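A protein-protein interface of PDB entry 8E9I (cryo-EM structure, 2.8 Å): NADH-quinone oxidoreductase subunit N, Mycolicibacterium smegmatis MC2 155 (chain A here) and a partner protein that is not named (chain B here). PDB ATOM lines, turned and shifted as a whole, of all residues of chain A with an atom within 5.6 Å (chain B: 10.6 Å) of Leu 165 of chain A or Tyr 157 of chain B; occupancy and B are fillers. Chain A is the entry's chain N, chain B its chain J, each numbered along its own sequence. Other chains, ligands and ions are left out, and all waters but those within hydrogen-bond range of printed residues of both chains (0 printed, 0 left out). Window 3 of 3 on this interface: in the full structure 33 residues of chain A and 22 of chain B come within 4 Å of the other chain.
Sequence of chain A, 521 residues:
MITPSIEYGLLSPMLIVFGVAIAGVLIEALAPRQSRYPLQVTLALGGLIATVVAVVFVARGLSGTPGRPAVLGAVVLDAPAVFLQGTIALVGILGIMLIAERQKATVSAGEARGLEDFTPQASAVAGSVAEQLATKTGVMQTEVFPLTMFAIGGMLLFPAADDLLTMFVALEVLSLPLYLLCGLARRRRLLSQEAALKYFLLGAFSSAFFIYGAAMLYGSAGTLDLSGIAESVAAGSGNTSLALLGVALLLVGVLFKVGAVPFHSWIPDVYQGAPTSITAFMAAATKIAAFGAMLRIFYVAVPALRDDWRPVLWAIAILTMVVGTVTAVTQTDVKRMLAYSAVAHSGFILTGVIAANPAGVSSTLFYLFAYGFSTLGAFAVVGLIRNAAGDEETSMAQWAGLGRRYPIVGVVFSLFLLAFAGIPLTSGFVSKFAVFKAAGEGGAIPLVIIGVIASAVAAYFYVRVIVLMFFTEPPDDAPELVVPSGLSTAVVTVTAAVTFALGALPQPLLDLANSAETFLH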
ATOM      1  N   VAL A  71      20.650 -28.684 -25.309  1.00  0.00           N
ATOM      2  CA  VAL A  71      19.654 -27.650 -25.048  1.00  0.00           C
ATOM      3  C   VAL A  71      19.816 -27.142 -23.621  1.00  0.00           C
ATOM      4  O   VAL A  71      18.832 -26.838 -22.940  1.00  0.00           O
ATOM      5  CB  VAL A  71      18.231 -28.178 -25.295  1.00  0.00           C
ATOM      6  CG1 VAL A  71      17.214 -27.053 -25.172  1.00  0.00           C
ATOM      7  CG2 VAL A  71      18.143 -28.839 -26.658  1.00  0.00           C
ATOM      8  N   ASP A 163      17.209 -35.412 -19.014  1.00  0.00           N
ATOM      9  CA  ASP A 163      16.596 -34.982 -17.768  1.00  0.00           C
ATOM     10  C   ASP A 163      15.210 -35.597 -17.650  1.00  0.00           C
ATOM     11  O   ASP A 163      14.632 -36.055 -18.637  1.00  0.00           O
ATOM     12  CB  ASP A 163      16.514 -33.454 -17.675  1.00  0.00           C
ATOM     13  CG  ASP A 163      15.622 -32.843 -18.731  1.00  0.00           C
ATOM     14  OD1 ASP A 163      14.737 -33.539 -19.265  1.00  0.00           O
ATOM     15  OD2 ASP A 163      15.798 -31.646 -19.023  1.00  0.00           O
ATOM     16  N   LEU A 164      14.679 -35.592 -16.426  1.00  0.00           N
ATOM     17  CA  LEU A 164      13.409 -36.260 -16.181  1.00  0.00           C
ATOM     18  C   LEU A 164      12.280 -35.641 -16.982  1.00  0.00           C
ATOM     19  O   LEU A 164      11.451 -36.367 -17.540  1.00  0.00           O
ATOM     20  CB  LEU A 164      13.075 -36.224 -14.695  1.00  0.00           C
ATOM     21  CG  LEU A 164      13.670 -37.361 -13.867  1.00  0.00           C
ATOM     22  CD1 LEU A 164      13.040 -38.688 -14.243  1.00  0.00           C
ATOM     23  CD2 LEU A 164      15.164 -37.412 -14.062  1.00  0.00           C
ATOM     24  N   LEU A 165      12.221 -34.313 -17.053  1.00  0.00           N
ATOM     25  CA  LEU A 165      11.118 -33.675 -17.759  1.00  0.00           C
ATOM     26  C   LEU A 165      11.119 -34.066 -19.230  1.00  0.00           C
ATOM     27  O   LEU A 165      10.068 -34.375 -19.803  1.00  0.00           O
ATOM     28  CB  LEU A 165      11.204 -32.158 -17.605  1.00  0.00           C
ATOM     29  CG  LEU A 165      10.114 -31.389 -18.350  1.00  0.00           C
ATOM     30  CD1 LEU A 165       8.746 -31.863 -17.907  1.00  0.00           C
ATOM     31  CD2 LEU A 165      10.258 -29.900 -18.140  1.00  0.00           C
ATOM     32  N   THR A 166      12.293 -34.058 -19.862  1.00  0.00           N
ATOM     33  CA  THR A 166      12.357 -34.405 -21.275  1.00  0.00           C
ATOM     34  C   THR A 166      12.014 -35.869 -21.501  1.00  0.00           C
ATOM     35  O   THR A 166      11.325 -36.204 -22.467  1.00  0.00           O
ATOM     36  CB  THR A 166      13.735 -34.093 -21.846  1.00  0.00           C
ATOM     37  OG1 THR A 166      14.100 -32.755 -21.500  1.00  0.00           O
ATOM     38  CG2 THR A 166      13.713 -34.223 -23.348  1.00  0.00           C
ATOM     39  N   MET A 167      12.484 -36.764 -20.631  1.00  0.00           N
ATOM     40  CA  MET A 167      12.091 -38.159 -20.786  1.00  0.00           C
ATOM     41  C   MET A 167      10.587 -38.317 -20.655  1.00  0.00           C
ATOM     42  O   MET A 167       9.975 -39.062 -21.418  1.00  0.00           O
ATOM     43  CB  MET A 167      12.794 -39.065 -19.779  1.00  0.00           C
ATOM     44  CG  MET A 167      14.283 -39.188 -19.971  1.00  0.00           C
ATOM     45  SD  MET A 167      15.016 -40.330 -18.790  1.00  0.00           S
ATOM     46  CE  MET A 167      14.955 -39.347 -17.303  1.00  0.00           C
ATOM     47  N   PHE A 168       9.972 -37.639 -19.688  1.00  0.00           N
ATOM     48  CA  PHE A 168       8.535 -37.800 -19.511  1.00  0.00           C
ATOM     49  C   PHE A 168       7.780 -37.262 -20.718  1.00  0.00           C
ATOM     50  O   PHE A 168       6.858 -37.914 -21.229  1.00  0.00           O
ATOM     51  CB  PHE A 168       8.092 -37.097 -18.231  1.00  0.00           C
ATOM     52  CG  PHE A 168       6.614 -37.130 -18.003  1.00  0.00           C
ATOM     53  CD1 PHE A 168       5.956 -38.338 -17.855  1.00  0.00           C
ATOM     54  CD2 PHE A 168       5.885 -35.962 -17.921  1.00  0.00           C
ATOM     55  CE1 PHE A 168       4.595 -38.378 -17.637  1.00  0.00           C
ATOM     56  CE2 PHE A 168       4.525 -35.996 -17.705  1.00  0.00           C
ATOM     57  CZ  PHE A 168       3.878 -37.207 -17.564  1.00  0.00           C
ATOM     58  N   VAL A 169       8.167 -36.081 -21.198  1.00  0.00           N
ATOM     59  CA  VAL A 169       7.502 -35.506 -22.360  1.00  0.00           C
ATOM     60  C   VAL A 169       7.673 -36.415 -23.566  1.00  0.00           C
ATOM     61  O   VAL A 169       6.727 -36.643 -24.324  1.00  0.00           O
ATOM     62  CB  VAL A 169       8.038 -34.093 -22.643  1.00  0.00           C
ATOM     63  CG1 VAL A 169       7.580 -33.625 -24.006  1.00  0.00           C
ATOM     64  CG2 VAL A 169       7.579 -33.129 -21.565  1.00  0.00           C
ATOM     65  N   ALA A 170       8.880 -36.942 -23.768  1.00  0.00           N
ATOM     66  CA  ALA A 170       9.122 -37.833 -24.893  1.00  0.00           C
ATOM     67  C   ALA A 170       8.330 -39.122 -24.752  1.00  0.00           C
ATOM     68  O   ALA A 170       7.831 -39.666 -25.740  1.00  0.00           O
ATOM     69  CB  ALA A 170      10.613 -38.136 -25.002  1.00  0.00           C
ATOM     70  N   LEU A 224      16.613 -32.097 -11.885  1.00  0.00           N
ATOM     71  CA  LEU A 224      16.069 -33.175 -12.694  1.00  0.00           C
ATOM     72  C   LEU A 224      16.899 -33.463 -13.938  1.00  0.00           C
ATOM     73  O   LEU A 224      16.516 -34.327 -14.731  1.00  0.00           O
ATOM     74  CB  LEU A 224      14.612 -32.873 -13.062  1.00  0.00           C
ATOM     75  CG  LEU A 224      14.292 -31.602 -13.847  1.00  0.00           C
ATOM     76  CD1 LEU A 224      14.498 -31.805 -15.330  1.00  0.00           C
ATOM     77  CD2 LEU A 224      12.867 -31.174 -13.562  1.00  0.00           C
ATOM     78  N   GLY B 148      10.021 -16.010 -13.371  1.00  0.00           N
ATOM     79  CA  GLY B 148      10.912 -17.141 -13.181  1.00  0.00           C
ATOM     80  C   GLY B 148      10.507 -18.339 -14.016  1.00  0.00           C
ATOM     81  O   GLY B 148      11.352 -19.025 -14.602  1.00  0.00           O
ATOM     82  N   LEU B 149       9.204 -18.612 -14.078  1.00  0.00           N
ATOM     83  CA  LEU B 149       8.747 -19.731 -14.897  1.00  0.00           C
ATOM     84  C   LEU B 149       9.073 -19.498 -16.363  1.00  0.00           C
ATOM     85  O   LEU B 149       9.431 -20.433 -17.081  1.00  0.00           O
ATOM     86  CB  LEU B 149       7.250 -19.953 -14.719  1.00  0.00           C
ATOM     87  CG  LEU B 149       6.800 -20.365 -13.322  1.00  0.00           C
ATOM     88  CD1 LEU B 149       5.298 -20.246 -13.231  1.00  0.00           C
ATOM     89  CD2 LEU B 149       7.259 -21.767 -12.984  1.00  0.00           C
ATOM     90  N   ALA B 150       8.938 -18.261 -16.834  1.00  0.00           N
ATOM     91  CA  ALA B 150       9.301 -17.960 -18.211  1.00  0.00           C
ATOM     92  C   ALA B 150      10.792 -18.159 -18.428  1.00  0.00           C
ATOM     93  O   ALA B 150      11.216 -18.735 -19.434  1.00  0.00           O
ATOM     94  CB  ALA B 150       8.890 -16.534 -18.559  1.00  0.00           C
ATOM     95  N   ALA B 151      11.607 -17.696 -17.479  1.00  0.00           N
ATOM     96  CA  ALA B 151      13.043 -17.900 -17.597  1.00  0.00           C
ATOM     97  C   ALA B 151      13.365 -19.376 -17.763  1.00  0.00           C
ATOM     98  O   ALA B 151      14.099 -19.761 -18.679  1.00  0.00           O
ATOM     99  CB  ALA B 151      13.759 -17.333 -16.374  1.00  0.00           C
ATOM    100  N   LEU B 152      12.801 -20.222 -16.905  1.00  0.00           N
ATOM    101  CA  LEU B 152      13.093 -21.651 -16.982  1.00  0.00           C
ATOM    102  C   LEU B 152      12.550 -22.262 -18.267  1.00  0.00           C
ATOM    103  O   LEU B 152      13.272 -22.952 -18.993  1.00  0.00           O
ATOM    104  CB  LEU B 152      12.502 -22.369 -15.775  1.00  0.00           C
ATOM    105  CG  LEU B 152      13.427 -22.581 -14.590  1.00  0.00           C
ATOM    106  CD1 LEU B 152      13.999 -21.265 -14.117  1.00  0.00           C
ATOM    107  CD2 LEU B 152      12.645 -23.248 -13.486  1.00  0.00           C
ATOM    108  N   ILE B 153      11.276 -22.014 -18.565  1.00  0.00           N
ATOM    109  CA  ILE B 153      10.593 -22.752 -19.623  1.00  0.00           C
ATOM    110  C   ILE B 153      11.272 -22.513 -20.961  1.00  0.00           C
ATOM    111  O   ILE B 153      11.503 -23.448 -21.736  1.00  0.00           O
ATOM    112  CB  ILE B 153       9.109 -22.354 -19.676  1.00  0.00           C
ATOM    113  CG1 ILE B 153       8.387 -22.816 -18.417  1.00  0.00           C
ATOM    114  CG2 ILE B 153       8.443 -22.954 -20.888  1.00  0.00           C
ATOM    115  CD1 ILE B 153       7.127 -22.035 -18.133  1.00  0.00           C
ATOM    116  N   PHE B 154      11.595 -21.259 -21.254  1.00  0.00           N
ATOM    117  CA  PHE B 154      12.114 -20.878 -22.556  1.00  0.00           C
ATOM    118  C   PHE B 154      13.631 -20.798 -22.579  1.00  0.00           C
ATOM    119  O   PHE B 154      14.202 -20.358 -23.583  1.00  0.00           O
ATOM    120  CB  PHE B 154      11.494 -19.548 -22.985  1.00  0.00           C
ATOM    121  CG  PHE B 154      10.000 -19.561 -22.948  1.00  0.00           C
ATOM    122  CD1 PHE B 154       9.281 -20.171 -23.955  1.00  0.00           C
ATOM    123  CD2 PHE B 154       9.314 -18.999 -21.891  1.00  0.00           C
ATOM    124  CE1 PHE B 154       7.911 -20.204 -23.920  1.00  0.00           C
ATOM    125  CE2 PHE B 154       7.938 -19.027 -21.852  1.00  0.00           C
ATOM    126  CZ  PHE B 154       7.237 -19.636 -22.866  1.00  0.00           C
ATOM    127  N   THR B 155      14.294 -21.200 -21.497  1.00  0.00           N
ATOM    128  CA  THR B 155      15.747 -21.269 -21.492  1.00  0.00           C
ATOM    129  C   THR B 155      16.231 -22.698 -21.290  1.00  0.00           C
ATOM    130  O   THR B 155      16.907 -23.255 -22.160  1.00  0.00           O
ATOM    131  CB  THR B 155      16.314 -20.363 -20.403  1.00  0.00           C
ATOM    132  OG1 THR B 155      15.818 -19.032 -20.589  1.00  0.00           O
ATOM    133  CG2 THR B 155      17.832 -20.351 -20.459  1.00  0.00           C
ATOM    134  N   ARG B 156      15.870 -23.310 -20.161  1.00  0.00           N
ATOM    135  CA  ARG B 156      16.377 -24.646 -19.860  1.00  0.00           C
ATOM    136  C   ARG B 156      15.448 -25.721 -20.401  1.00  0.00           C
ATOM    137  O   ARG B 156      15.907 -26.743 -20.918  1.00  0.00           O
ATOM    138  CB  ARG B 156      16.560 -24.813 -18.353  1.00  0.00           C
ATOM    139  N   TYR B 157      14.140 -25.511 -20.282  1.00  0.00           N
ATOM    140  CA  TYR B 157      13.146 -26.487 -20.706  1.00  0.00           C
ATOM    141  C   TYR B 157      12.535 -26.133 -22.054  1.00  0.00           C
ATOM    142  O   TYR B 157      11.369 -26.448 -22.308  1.00  0.00           O
ATOM    143  CB  TYR B 157      12.064 -26.602 -19.636  1.00  0.00           C
ATOM    144  CG  TYR B 157      12.628 -26.993 -18.302  1.00  0.00           C
ATOM    145  CD1 TYR B 157      13.224 -28.229 -18.116  1.00  0.00           C
ATOM    146  CD2 TYR B 157      12.612 -26.111 -17.239  1.00  0.00           C
ATOM    147  CE1 TYR B 157      13.752 -28.590 -16.903  1.00  0.00           C
ATOM    148  CE2 TYR B 157      13.142 -26.462 -16.020  1.00  0.00           C
ATOM    149  CZ  TYR B 157      13.713 -27.703 -15.857  1.00  0.00           C
ATOM    150  OH  TYR B 157      14.245 -28.058 -14.642  1.00  0.00           O
ATOM    151  N   LEU B 158      13.304 -25.482 -22.925  1.00  0.00           N
ATOM    152  CA  LEU B 158      12.777 -25.078 -24.221  1.00  0.00           C
ATOM    153  C   LEU B 158      12.412 -26.289 -25.068  1.00  0.00           C
ATOM    154  O   LEU B 158      11.402 -26.281 -25.778  1.00  0.00           O
ATOM    155  CB  LEU B 158      13.802 -24.202 -24.939  1.00  0.00           C
ATOM    156  CG  LEU B 158      13.601 -23.989 -26.436  1.00  0.00           C
ATOM    157  CD1 LEU B 158      12.247 -23.366 -26.701  1.00  0.00           C
ATOM    158  CD2 LEU B 158      14.710 -23.111 -26.985  1.00  0.00           C
ATOM    159  N   TRP B 159      13.227 -27.341 -25.009  1.00  0.00           N
ATOM    160  CA  TRP B 159      12.973 -28.520 -25.829  1.00  0.00           C
ATOM    161  C   TRP B 159      11.663 -29.194 -25.438  1.00  0.00           C
ATOM    162  O   TRP B 159      10.856 -29.563 -26.303  1.00  0.00           O
ATOM    163  CB  TRP B 159      14.153 -29.485 -25.704  1.00  0.00           C
ATOM    164  CG  TRP B 159      14.275 -30.439 -26.834  1.00  0.00           C
ATOM    165  CD1 TRP B 159      14.333 -31.795 -26.753  1.00  0.00           C
ATOM    166  CD2 TRP B 159      14.340 -30.116 -28.224  1.00  0.00           C
ATOM    167  NE1 TRP B 159      14.439 -32.340 -28.006  1.00  0.00           N
ATOM    168  CE2 TRP B 159      14.445 -31.329 -28.929  1.00  0.00           C
ATOM    169  CE3 TRP B 159      14.321 -28.919 -28.943  1.00  0.00           C
ATOM    170  CZ2 TRP B 159      14.530 -31.381 -30.313  1.00  0.00           C
ATOM    171  CZ3 TRP B 159      14.406 -28.971 -30.316  1.00  0.00           C
ATOM    172  CH2 TRP B 159      14.508 -30.195 -30.988  1.00  0.00           C
ATOM    173  N   ALA B 160      11.424 -29.354 -24.136  1.00  0.00           N
ATOM    174  CA  ALA B 160      10.169 -29.940 -23.681  1.00  0.00           C
ATOM    175  C   ALA B 160       8.989 -29.063 -24.075  1.00  0.00           C
ATOM    176  O   ALA B 160       7.919 -29.560 -24.450  1.00  0.00           O
ATOM    177  CB  ALA B 160      10.212 -30.144 -22.169  1.00  0.00           C
ATOM    178  N   PHE B 161       9.163 -27.747 -23.980  1.00  0.00           N
ATOM    179  CA  PHE B 161       8.112 -26.827 -24.389  1.00  0.00           C
ATOM    180  C   PHE B 161       7.783 -27.010 -25.862  1.00  0.00           C
ATOM    181  O   PHE B 161       6.618 -26.956 -26.267  1.00  0.00           O
ATOM    182  CB  PHE B 161       8.544 -25.392 -24.103  1.00  0.00           C
ATOM    183  CG  PHE B 161       7.778 -24.369 -24.875  1.00  0.00           C
ATOM    184  CD1 PHE B 161       6.412 -24.253 -24.725  1.00  0.00           C
ATOM    185  CD2 PHE B 161       8.424 -23.521 -25.748  1.00  0.00           C
ATOM    186  CE1 PHE B 161       5.706 -23.310 -25.435  1.00  0.00           C
ATOM    187  CE2 PHE B 161       7.721 -22.576 -26.456  1.00  0.00           C
ATOM    188  CZ  PHE B 161       6.361 -22.472 -26.298  1.00  0.00           C
ATOM    189  N   GLU B 162       8.809 -27.208 -26.686  1.00  0.00           N
ATOM    190  CA  GLU B 162       8.569 -27.455 -28.100  1.00  0.00           C
ATOM    191  C   GLU B 162       7.822 -28.764 -28.305  1.00  0.00           C
ATOM    192  O   GLU B 162       6.896 -28.840 -29.120  1.00  0.00           O
ATOM    193  CB  GLU B 162       9.893 -27.465 -28.859  1.00  0.00           C
ATOM    194  N   LEU B 163       8.202 -29.804 -27.565  1.00  0.00           N
ATOM    195  CA  LEU B 163       7.559 -31.105 -27.728  1.00  0.00           C
ATOM    196  C   LEU B 163       6.115 -31.110 -27.246  1.00  0.00           C
ATOM    197  O   LEU B 163       5.328 -31.973 -27.663  1.00  0.00           O
ATOM    198  CB  LEU B 163       8.353 -32.164 -26.985  1.00  0.00           C
ATOM    199  CG  LEU B 163       9.754 -32.342 -27.555  1.00  0.00           C
ATOM    200  CD1 LEU B 163      10.712 -32.760 -26.464  1.00  0.00           C
ATOM    201  CD2 LEU B 163       9.720 -33.358 -28.681  1.00  0.00           C
ATOM    202  N   THR B 164       5.749 -30.193 -26.357  1.00  0.00           N
ATOM    203  CA  THR B 164       4.335 -30.060 -26.032  1.00  0.00           C
ATOM    204  C   THR B 164       3.514 -29.809 -27.287  1.00  0.00           C
ATOM    205  O   THR B 164       2.349 -30.216 -27.361  1.00  0.00           O
ATOM    206  CB  THR B 164       4.111 -28.935 -25.031  1.00  0.00           C
ATOM    207  OG1 THR B 164       4.652 -27.720 -25.557  1.00  0.00           O
ATOM    208  CG2 THR B 164       4.763 -29.269 -23.702  1.00  0.00           C
ATOM    209  N   SER B 165       4.098 -29.149 -28.286  1.00  0.00           N
ATOM    210  CA  SER B 165       3.396 -28.971 -29.549  1.00  0.00           C
ATOM    211  C   SER B 165       3.146 -30.307 -30.227  1.00  0.00           C
ATOM    212  O   SER B 165       2.081 -30.515 -30.818  1.00  0.00           O
ATOM    213  CB  SER B 165       4.194 -28.055 -30.473  1.00  0.00           C
ATOM    214  OG  SER B 165       5.312 -28.734 -31.013  1.00  0.00           O
ATOM    215  N   LEU B 167       2.734 -33.114 -28.652  1.00  0.00           N
ATOM    216  CA  LEU B 167       1.628 -33.687 -27.887  1.00  0.00           C
ATOM    217  C   LEU B 167       0.293 -33.129 -28.367  1.00  0.00           C
ATOM    218  O   LEU B 167      -0.665 -33.877 -28.600  1.00  0.00           O
ATOM    219  CB  LEU B 167       1.814 -33.411 -26.396  1.00  0.00           C
ATOM    220  CG  LEU B 167       2.976 -34.097 -25.688  1.00  0.00           C
ATOM    221  CD1 LEU B 167       3.139 -33.541 -24.291  1.00  0.00           C
ATOM    222  CD2 LEU B 167       2.743 -35.588 -25.638  1.00  0.00           C
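Among the printed residues, pairs that only touch across the chains: Val 71 of chain A with Arg 156 of chain B, Val 71 of chain A with Trp 159 of chain B, Leu 165 of chain A with Tyr 157 of chain B, Val 169 of chain A with Leu 163 of chain B and Leu 224 of chain A with Tyr 157 of chain B.
Of the printed residues of chain B, Leu 165 of chain A touches Tyr 157. Tyr 157 of chain B touches two residues of chain A. No residue of chain B comes within 4 Å of Asp 163 of chain A. No residue of chain B comes within 4 Å of Leu 164 of chain A. No residue of chain B comes within 4 Å of Thr 166 of chain A. Of chain B, only Leu 163 (3.4 Å) comes within 4 Å of Val 169 of chain A. Of the printed residues of chain A, Leu 163 of chain B touches Val 169. Printed residues of chain A within 4 Å of Arg 156 of chain B: Val 71. Of the printed residues of chain B, Val 71 of chain A touches Arg 156 (3.6 Å) and Trp 159 (3.9 Å). Of the printed residues of chain A, Trp 159 of chain B touches Val 71 (3.9 Å). Leu 152 of chain B touches none of the printed residues of chain A. Leu 149 of chain B touches none of the printed residues of chain A. The nearest residue of chain A that does not touch Tyr 157 of chain B is Asp 163 of chain A (4.2 Å). The nearest printed residue of chain B that does not touch Val 71 of chain A is Thr 155 of chain B (4.1 Å).
N of Tyr 157 of chain B lies within hydrogen-bond range of O of Leu 152 of chain B (3.0 Å). The backbone NH (N) of Leu 165 of chain A sits close to the side-chain carboxylate (OD1) of Asp 163 of chain A. The backbone NH (N) of Leu 164 of chain A is in hydrogen-bond range of the backbone carbonyl oxygen (O) of Leu 224 of chain A (2.8 Å).
Along chain B the printed residues that touch a printed residue of chain A span positions 156 to 163. Of the 10 printed residues of chain A, 4 touch a printed residue of chain B. Along chain A the printed residues that touch a printed residue of chain B span positions 71 to 224.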
